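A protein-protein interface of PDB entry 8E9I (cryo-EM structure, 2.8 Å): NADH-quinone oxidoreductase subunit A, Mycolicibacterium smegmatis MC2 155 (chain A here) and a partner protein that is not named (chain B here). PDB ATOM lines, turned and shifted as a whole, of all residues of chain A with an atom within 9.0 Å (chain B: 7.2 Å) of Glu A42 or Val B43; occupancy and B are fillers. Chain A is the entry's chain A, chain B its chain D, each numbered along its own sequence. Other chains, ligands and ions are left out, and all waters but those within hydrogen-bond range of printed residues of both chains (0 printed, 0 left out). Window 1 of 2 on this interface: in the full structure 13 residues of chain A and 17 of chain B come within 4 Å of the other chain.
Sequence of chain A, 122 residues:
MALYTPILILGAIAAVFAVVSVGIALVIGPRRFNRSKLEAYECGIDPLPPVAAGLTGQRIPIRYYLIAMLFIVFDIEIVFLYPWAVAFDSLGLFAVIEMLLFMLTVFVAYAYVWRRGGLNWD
O of Met B45 sits at hydrogen-bond distance from SG of Cys A43. The backbone carbonyl oxygen (O) of Cys A43 sits at hydrogen-bond distance from the backbone NH (N) of Gln B48, 3.3 Å away. OE2 of Glu A42 sits at hydrogen-bond distance from N of Asn B44 (2.5 Å). The backbone carbonyl oxygen (O) of Asn B44 is in hydrogen-bond range of the side-chain sulfur (SG) of Cys A43, at 3.5 Å. OH of Tyr A41 sits at hydrogen-bond distance from O of Gln B48, at 2.6 Å.
OD1 of Asn B44 sits at hydrogen-bond distance from NE of Arg B57. O of Val B43 sits at hydrogen-bond distance from N of Leu B60. The side-chain sulfur of Cys A43 lies close to the side-chain hydroxyl of Tyr A41, 3.4 Å away. The backbone NH (N) of Met B45 lies within hydrogen-bond range of the backbone carbonyl oxygen (O) of Leu B58.
Among the printed residues, pairs that only touch across the chains: Glu A42 with Val B43, Cys A43 with Gly B46, Cys A43 with Pro B47, Ile A45 with Asn B44, Ile A45 with Pro B47, Ile A45 with Arg B57 and Leu A48 with Val B42.
Of chain B, only Val B43 (3.2 Å) and Asn B44 (2.5 Å) come within 4 Å of Glu A42. Printed residues of chain B within 4 Å of Cys A43: Asn B44 (3.5 Å), Met B45 (3.6 Å), Gly B46 (3.6 Å), Pro B47 (3.5 Å) and Gln B48 (3.3 Å). Pro A47 touches none of the printed residues of chain B. Ile B41 touches none of the printed residues of chain A. Of the printed residues of chain A, Val B42 touches Leu A48 (3.9 Å). Val B43 touches just one residue of chain A: Glu A42 (3.2 Å). Of the printed residues of chain A, Gln B48 touches Tyr A41 (2.4 Å) and Cys A43 (3.3 Å).
Of the 18 printed residues of chain B, 8 touch a printed residue of chain A. Hydrophobic or aromatic side chains of chain B that line the printed part of chain A: Val B42, Val B43 and Pro B47. Of the 11 printed residues of chain A, 5 touch a printed residue of chain B. Among the printed residues, 12 pairs touch across the chains.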
ATOM      1  N   SER A  36      29.937  -0.857  31.828  1.00  0.00           N
ATOM      2  CA  SER A  36      29.548  -1.797  30.783  1.00  0.00           C
ATOM      3  C   SER A  36      30.689  -2.748  30.446  1.00  0.00           C
ATOM      4  O   SER A  36      30.481  -3.954  30.284  1.00  0.00           O
ATOM      5  CB  SER A  36      29.100  -1.033  29.538  1.00  0.00           C
ATOM      6  OG  SER A  36      28.587  -1.913  28.556  1.00  0.00           O
ATOM      7  N   GLU A  39      31.058  -5.372  33.166  1.00  0.00           N
ATOM      8  CA  GLU A  39      29.937  -6.264  33.395  1.00  0.00           C
ATOM      9  C   GLU A  39      30.179  -7.602  32.701  1.00  0.00           C
ATOM     10  O   GLU A  39      30.963  -7.715  31.756  1.00  0.00           O
ATOM     11  CB  GLU A  39      28.638  -5.631  32.902  1.00  0.00           C
ATOM     12  N   ALA A  40      29.488  -8.629  33.181  1.00  0.00           N
ATOM     13  CA  ALA A  40      29.640  -9.954  32.606  1.00  0.00           C
ATOM     14  C   ALA A  40      29.272  -9.929  31.132  1.00  0.00           C
ATOM     15  O   ALA A  40      28.423  -9.150  30.695  1.00  0.00           O
ATOM     16  CB  ALA A  40      28.759 -10.961  33.345  1.00  0.00           C
ATOM     17  N   TYR A  41      29.936 -10.776  30.354  1.00  0.00           N
ATOM     18  CA  TYR A  41      29.558 -10.928  28.959  1.00  0.00           C
ATOM     19  C   TYR A  41      28.318 -11.801  28.865  1.00  0.00           C
ATOM     20  O   TYR A  41      28.287 -12.911  29.402  1.00  0.00           O
ATOM     21  CB  TYR A  41      30.692 -11.545  28.151  1.00  0.00           C
ATOM     22  CG  TYR A  41      30.276 -11.929  26.758  1.00  0.00           C
ATOM     23  CD1 TYR A  41      30.050 -10.964  25.794  1.00  0.00           C
ATOM     24  CD2 TYR A  41      30.107 -13.256  26.406  1.00  0.00           C
ATOM     25  CE1 TYR A  41      29.665 -11.305  24.525  1.00  0.00           C
ATOM     26  CE2 TYR A  41      29.726 -13.606  25.139  1.00  0.00           C
ATOM     27  CZ  TYR A  41      29.510 -12.627  24.201  1.00  0.00           C
ATOM     28  OH  TYR A  41      29.127 -12.967  22.929  1.00  0.00           O
ATOM     29  N   GLU A  42      27.293 -11.298  28.188  1.00  0.00           N
ATOM     30  CA  GLU A  42      26.070 -12.056  27.961  1.00  0.00           C
ATOM     31  C   GLU A  42      25.615 -11.860  26.521  1.00  0.00           C
ATOM     32  O   GLU A  42      24.437 -11.652  26.236  1.00  0.00           O
ATOM     33  CB  GLU A  42      24.983 -11.640  28.946  1.00  0.00           C
ATOM     34  CG  GLU A  42      23.774 -12.555  28.976  1.00  0.00           C
ATOM     35  CD  GLU A  42      24.133 -13.997  29.266  1.00  0.00           C
ATOM     36  OE1 GLU A  42      25.118 -14.228  29.994  1.00  0.00           O
ATOM     37  OE2 GLU A  42      23.429 -14.898  28.775  1.00  0.00           O
ATOM     38  N   CYS A  43      26.566 -11.910  25.594  1.00  0.00           N
ATOM     39  CA  CYS A  43      26.282 -11.770  24.170  1.00  0.00           C
ATOM     40  C   CYS A  43      25.649 -10.424  23.845  1.00  0.00           C
ATOM     41  O   CYS A  43      24.969 -10.280  22.828  1.00  0.00           O
ATOM     42  CB  CYS A  43      25.393 -12.914  23.684  1.00  0.00           C
ATOM     43  SG  CYS A  43      26.202 -14.516  23.755  1.00  0.00           S
ATOM     44  N   GLY A  44      25.877  -9.419  24.694  1.00  0.00           N
ATOM     45  CA  GLY A  44      25.427  -8.063  24.467  1.00  0.00           C
ATOM     46  C   GLY A  44      24.198  -7.685  25.266  1.00  0.00           C
ATOM     47  O   GLY A  44      23.866  -6.497  25.348  1.00  0.00           O
ATOM     48  N   ILE A  45      23.515  -8.665  25.854  1.00  0.00           N
ATOM     49  CA  ILE A  45      22.331  -8.380  26.648  1.00  0.00           C
ATOM     50  C   ILE A  45      22.743  -7.964  28.050  1.00  0.00           C
ATOM     51  O   ILE A  45      23.790  -8.382  28.563  1.00  0.00           O
ATOM     52  CB  ILE A  45      21.409  -9.609  26.679  1.00  0.00           C
ATOM     53  CG1 ILE A  45      20.937  -9.959  25.268  1.00  0.00           C
ATOM     54  CG2 ILE A  45      20.223  -9.363  27.581  1.00  0.00           C
ATOM     55  CD1 ILE A  45      20.358  -8.799  24.496  1.00  0.00           C
ATOM     56  N   ASP A  46      21.922  -7.139  28.680  1.00  0.00           N
ATOM     57  CA  ASP A  46      22.213  -6.714  30.038  1.00  0.00           C
ATOM     58  C   ASP A  46      22.268  -7.934  30.956  1.00  0.00           C
ATOM     59  O   ASP A  46      21.326  -8.735  30.975  1.00  0.00           O
ATOM     60  CB  ASP A  46      21.146  -5.734  30.530  1.00  0.00           C
ATOM     61  N   PRO A  47      23.346  -8.120  31.717  1.00  0.00           N
ATOM     62  CA  PRO A  47      23.380  -9.238  32.661  1.00  0.00           C
ATOM     63  C   PRO A  47      22.370  -9.032  33.776  1.00  0.00           C
ATOM     64  O   PRO A  47      22.005  -7.904  34.113  1.00  0.00           O
ATOM     65  CB  PRO A  47      24.816  -9.215  33.186  1.00  0.00           C
ATOM     66  CG  PRO A  47      25.245  -7.815  33.021  1.00  0.00           C
ATOM     67  CD  PRO A  47      24.584  -7.325  31.773  1.00  0.00           C
ATOM     68  N   LEU A  48      21.928 -10.137  34.355  1.00  0.00           N
ATOM     69  CA  LEU A  48      20.865 -10.125  35.349  1.00  0.00           C
ATOM     70  C   LEU A  48      21.139  -9.137  36.472  1.00  0.00           C
ATOM     71  O   LEU A  48      22.275  -8.675  36.636  1.00  0.00           O
ATOM     72  CB  LEU A  48      20.691 -11.522  35.933  1.00  0.00           C
ATOM     73  CG  LEU A  48      19.963 -12.518  35.045  1.00  0.00           C
ATOM     74  CD1 LEU A  48      20.097 -13.912  35.620  1.00  0.00           C
ATOM     75  CD2 LEU A  48      18.503 -12.123  34.930  1.00  0.00           C
ATOM     76  N   ILE B  41      19.723 -22.324  35.052  1.00  0.00           N
ATOM     77  CA  ILE B  41      20.232 -21.015  34.669  1.00  0.00           C
ATOM     78  C   ILE B  41      19.434 -20.491  33.481  1.00  0.00           C
ATOM     79  O   ILE B  41      18.840 -21.248  32.716  1.00  0.00           O
ATOM     80  CB  ILE B  41      21.733 -21.084  34.338  1.00  0.00           C
ATOM     81  CG1 ILE B  41      22.487 -21.814  35.447  1.00  0.00           C
ATOM     82  CG2 ILE B  41      22.300 -19.694  34.120  1.00  0.00           C
ATOM     83  CD1 ILE B  41      22.662 -23.294  35.185  1.00  0.00           C
ATOM     84  N   VAL B  42      19.414 -19.173  33.330  1.00  0.00           N
ATOM     85  CA  VAL B  42      18.828 -18.531  32.161  1.00  0.00           C
ATOM     86  C   VAL B  42      19.928 -17.756  31.455  1.00  0.00           C
ATOM     87  O   VAL B  42      20.546 -16.865  32.046  1.00  0.00           O
ATOM     88  CB  VAL B  42      17.653 -17.608  32.534  1.00  0.00           C
ATOM     89  CG1 VAL B  42      18.070 -16.600  33.587  1.00  0.00           C
ATOM     90  CG2 VAL B  42      17.131 -16.908  31.299  1.00  0.00           C
ATOM     91  N   VAL B  43      20.174 -18.098  30.197  1.00  0.00           N
ATOM     92  CA  VAL B  43      21.314 -17.580  29.456  1.00  0.00           C
ATOM     93  C   VAL B  43      20.825 -17.050  28.119  1.00  0.00           C
ATOM     94  O   VAL B  43      19.762 -17.442  27.632  1.00  0.00           O
ATOM     95  CB  VAL B  43      22.392 -18.665  29.256  1.00  0.00           C
ATOM     96  CG1 VAL B  43      21.840 -19.817  28.447  1.00  0.00           C
ATOM     97  CG2 VAL B  43      23.622 -18.090  28.587  1.00  0.00           C
ATOM     98  N   ASN B  44      21.590 -16.135  27.540  1.00  0.00           N
ATOM     99  CA  ASN B  44      21.346 -15.658  26.185  1.00  0.00           C
ATOM    100  C   ASN B  44      22.355 -16.311  25.254  1.00  0.00           C
ATOM    101  O   ASN B  44      23.557 -16.050  25.356  1.00  0.00           O
ATOM    102  CB  ASN B  44      21.471 -14.139  26.111  1.00  0.00           C
ATOM    103  CG  ASN B  44      20.509 -13.429  27.022  1.00  0.00           C
ATOM    104  OD1 ASN B  44      19.453 -12.969  26.593  1.00  0.00           O
ATOM    105  ND2 ASN B  44      20.856 -13.352  28.295  1.00  0.00           N
ATOM    106  N   MET B  45      21.877 -17.156  24.341  1.00  0.00           N
ATOM    107  CA  MET B  45      22.636 -17.354  23.116  1.00  0.00           C
ATOM    108  C   MET B  45      22.782 -16.024  22.402  1.00  0.00           C
ATOM    109  O   MET B  45      23.672 -15.845  21.569  1.00  0.00           O
ATOM    110  CB  MET B  45      21.957 -18.371  22.208  1.00  0.00           C
ATOM    111  CG  MET B  45      21.894 -19.785  22.746  1.00  0.00           C
ATOM    112  SD  MET B  45      23.523 -20.499  23.015  1.00  0.00           S
ATOM    113  CE  MET B  45      23.668 -20.338  24.789  1.00  0.00           C
ATOM    114  N   GLY B  46      21.889 -15.088  22.700  1.00  0.00           N
ATOM    115  CA  GLY B  46      22.129 -13.689  22.472  1.00  0.00           C
ATOM    116  C   GLY B  46      22.313 -13.350  21.016  1.00  0.00           C
ATOM    117  O   GLY B  46      22.518 -14.223  20.168  1.00  0.00           O
ATOM    118  N   PRO B  47      22.240 -12.079  20.694  1.00  0.00           N
ATOM    119  CA  PRO B  47      22.530 -11.670  19.320  1.00  0.00           C
ATOM    120  C   PRO B  47      23.972 -11.959  18.951  1.00  0.00           C
ATOM    121  O   PRO B  47      24.237 -12.680  17.987  1.00  0.00           O
ATOM    122  CB  PRO B  47      22.221 -10.168  19.330  1.00  0.00           C
ATOM    123  CG  PRO B  47      21.295  -9.988  20.488  1.00  0.00           C
ATOM    124  CD  PRO B  47      21.778 -10.947  21.510  1.00  0.00           C
ATOM    125  N   GLN B  48      24.913 -11.430  19.727  1.00  0.00           N
ATOM    126  CA  GLN B  48      26.333 -11.554  19.407  1.00  0.00           C
ATOM    127  C   GLN B  48      26.816 -12.909  19.894  1.00  0.00           C
ATOM    128  O   GLN B  48      27.328 -13.053  21.003  1.00  0.00           O
ATOM    129  CB  GLN B  48      27.135 -10.423  20.037  1.00  0.00           C
ATOM    130  CG  GLN B  48      28.511 -10.262  19.429  1.00  0.00           C
ATOM    131  CD  GLN B  48      29.498 -11.282  19.947  1.00  0.00           C
ATOM    132  OE1 GLN B  48      29.644 -11.469  21.152  1.00  0.00           O
ATOM    133  NE2 GLN B  48      30.168 -11.967  19.033  1.00  0.00           N
ATOM    134  N   ARG B  57      18.327 -14.033  19.032  1.00  0.00           N
ATOM    135  CA  ARG B  57      18.524 -14.159  20.476  1.00  0.00           C
ATOM    136  C   ARG B  57      17.779 -15.382  21.005  1.00  0.00           C
ATOM    137  O   ARG B  57      16.571 -15.352  21.193  1.00  0.00           O
ATOM    138  CB  ARG B  57      18.074 -12.894  21.184  1.00  0.00           C
ATOM    139  CG  ARG B  57      18.330 -12.909  22.675  1.00  0.00           C
ATOM    140  CD  ARG B  57      17.713 -11.707  23.337  1.00  0.00           C
ATOM    141  NE  ARG B  57      17.778 -11.778  24.789  1.00  0.00           N
ATOM    142  CZ  ARG B  57      17.217 -10.894  25.599  1.00  0.00           C
ATOM    143  NH1 ARG B  57      16.570  -9.842  25.130  1.00  0.00           N
ATOM    144  NH2 ARG B  57      17.306 -11.069  26.912  1.00  0.00           N
ATOM    145  N   LEU B  58      18.506 -16.457  21.269  1.00  0.00           N
ATOM    146  CA  LEU B  58      17.890 -17.592  21.943  1.00  0.00           C
ATOM    147  C   LEU B  58      18.085 -17.477  23.449  1.00  0.00           C
ATOM    148  O   LEU B  58      19.208 -17.571  23.951  1.00  0.00           O
ATOM    149  CB  LEU B  58      18.471 -18.901  21.422  1.00  0.00           C
ATOM    150  CG  LEU B  58      17.863 -19.385  20.112  1.00  0.00           C
ATOM    151  CD1 LEU B  58      18.287 -18.491  18.986  1.00  0.00           C
ATOM    152  CD2 LEU B  58      18.280 -20.815  19.839  1.00  0.00           C
ATOM    153  N   ILE B  59      16.987 -17.276  24.170  1.00  0.00           N
ATOM    154  CA  ILE B  59      16.990 -17.220  25.625  1.00  0.00           C
ATOM    155  C   ILE B  59      16.719 -18.631  26.117  1.00  0.00           C
ATOM    156  O   ILE B  59      15.606 -19.144  25.958  1.00  0.00           O
ATOM    157  CB  ILE B  59      15.939 -16.236  26.163  1.00  0.00           C
ATOM    158  CG1 ILE B  59      16.028 -14.899  25.428  1.00  0.00           C
ATOM    159  CG2 ILE B  59      16.127 -16.007  27.640  1.00  0.00           C
ATOM    160  CD1 ILE B  59      15.023 -14.751  24.311  1.00  0.00           C
ATOM    161  N   LEU B  60      17.727 -19.260  26.708  1.00  0.00           N
ATOM    162  CA  LEU B  60      17.656 -20.666  27.080  1.00  0.00           C
ATOM    163  C   LEU B  60      17.588 -20.802  28.592  1.00  0.00           C
ATOM    164  O   LEU B  60      18.442 -20.266  29.306  1.00  0.00           O
ATOM    165  CB  LEU B  60      18.857 -21.437  26.537  1.00  0.00           C
ATOM    166  CG  LEU B  60      19.145 -21.280  25.047  1.00  0.00           C
ATOM    167  CD1 LEU B  60      20.282 -22.190  24.640  1.00  0.00           C
ATOM    168  CD2 LEU B  60      17.908 -21.574  24.231  1.00  0.00           C
ATOM    169  N   GLU B  61      16.564 -21.500  29.070  1.00  0.00           N
ATOM    170  CA  GLU B  61      16.557 -21.984  30.441  1.00  0.00           C
ATOM    171  C   GLU B  61      17.140 -23.386  30.460  1.00  0.00           C
ATOM    172  O   GLU B  61      16.553 -24.319  29.908  1.00  0.00           O
ATOM    173  CB  GLU B  61      15.139 -21.985  31.004  1.00  0.00           C
ATOM    174  N   ILE B  62      18.304 -23.534  31.085  1.00  0.00           N
ATOM    175  CA  ILE B  62      19.108 -24.743  30.979  1.00  0.00           C
ATOM    176  C   ILE B  62      19.302 -25.333  32.366  1.00  0.00           C
ATOM    177  O   ILE B  62      19.696 -24.625  33.298  1.00  0.00           O
ATOM    178  CB  ILE B  62      20.463 -24.454  30.307  1.00  0.00           C
ATOM    179  CG1 ILE B  62      21.309 -23.511  31.163  1.00  0.00           C
ATOM    180  CG2 ILE B  62      20.240 -23.839  28.944  1.00  0.00           C
ATOM    181  CD1 ILE B  62      22.597 -23.088  30.504  1.00  0.00           C
ATOM    182  N   ILE B  67      18.741 -28.039  27.551  1.00  0.00           N
ATOM    183  CA  ILE B  67      17.799 -26.961  27.273  1.00  0.00           C
ATOM    184  C   ILE B  67      16.435 -27.346  27.829  1.00  0.00           C
ATOM    185  O   ILE B  67      15.837 -28.342  27.408  1.00  0.00           O
ATOM    186  CB  ILE B  67      17.717 -26.677  25.769  1.00  0.00           C
ATOM    187  CG1 ILE B  67      19.112 -26.504  25.164  1.00  0.00           C
ATOM    188  CG2 ILE B  67      16.873 -25.448  25.515  1.00  0.00           C
ATOM    189  CD1 ILE B  67      20.012 -25.590  25.943  1.00  0.00           C
ATOM    190  N   GLU B  69      13.806 -24.730  28.308  1.00  0.00           N
ATOM    191  CA  GLU B  69      12.935 -23.902  27.487  1.00  0.00           C
ATOM    192  C   GLU B  69      13.802 -23.042  26.583  1.00  0.00           C
ATOM    193  O   GLU B  69      14.895 -22.631  26.977  1.00  0.00           O
ATOM    194  CB  GLU B  69      12.029 -23.008  28.342  1.00  0.00           C
ATOM    195  N   ARG B  71      13.155 -19.738  24.569  1.00  0.00           N
ATOM    196  CA  ARG B  71      12.480 -18.559  24.057  1.00  0.00           C
ATOM    197  C   ARG B  71      13.292 -17.958  22.920  1.00  0.00           C
ATOM    198  O   ARG B  71      14.519 -18.048  22.890  1.00  0.00           O
ATOM    199  CB  ARG B  71      12.286 -17.534  25.169  1.00  0.00           C
ATOM    200  CG  ARG B  71      11.199 -17.912  26.143  1.00  0.00           C
ATOM    201  CD  ARG B  71      11.065 -16.902  27.252  1.00  0.00           C
ATOM    202  NE  ARG B  71       9.950 -17.241  28.125  1.00  0.00           N
ATOM    203  CZ  ARG B  71       9.993 -18.179  29.060  1.00  0.00           C
ATOM    204  NH1 ARG B  71      11.097 -18.866  29.300  1.00  0.00           N
ATOM    205  NH2 ARG B  71       8.899 -18.437  29.770  1.00  0.00           N
ATOM    206  N   VAL B 423      22.654 -28.219  24.809  1.00  0.00           N
ATOM    207  CA  VAL B 423      22.880 -26.916  24.193  1.00  0.00           C
ATOM    208  C   VAL B 423      23.715 -27.063  22.928  1.00  0.00           C
ATOM    209  O   VAL B 423      23.440 -26.411  21.912  1.00  0.00           O
ATOM    210  CB  VAL B 423      23.535 -25.951  25.201  1.00  0.00           C
ATOM    211  CG1 VAL B 423      24.957 -26.370  25.503  1.00  0.00           C
ATOM    212  CG2 VAL B 423      23.499 -24.541  24.669  1.00  0.00           C
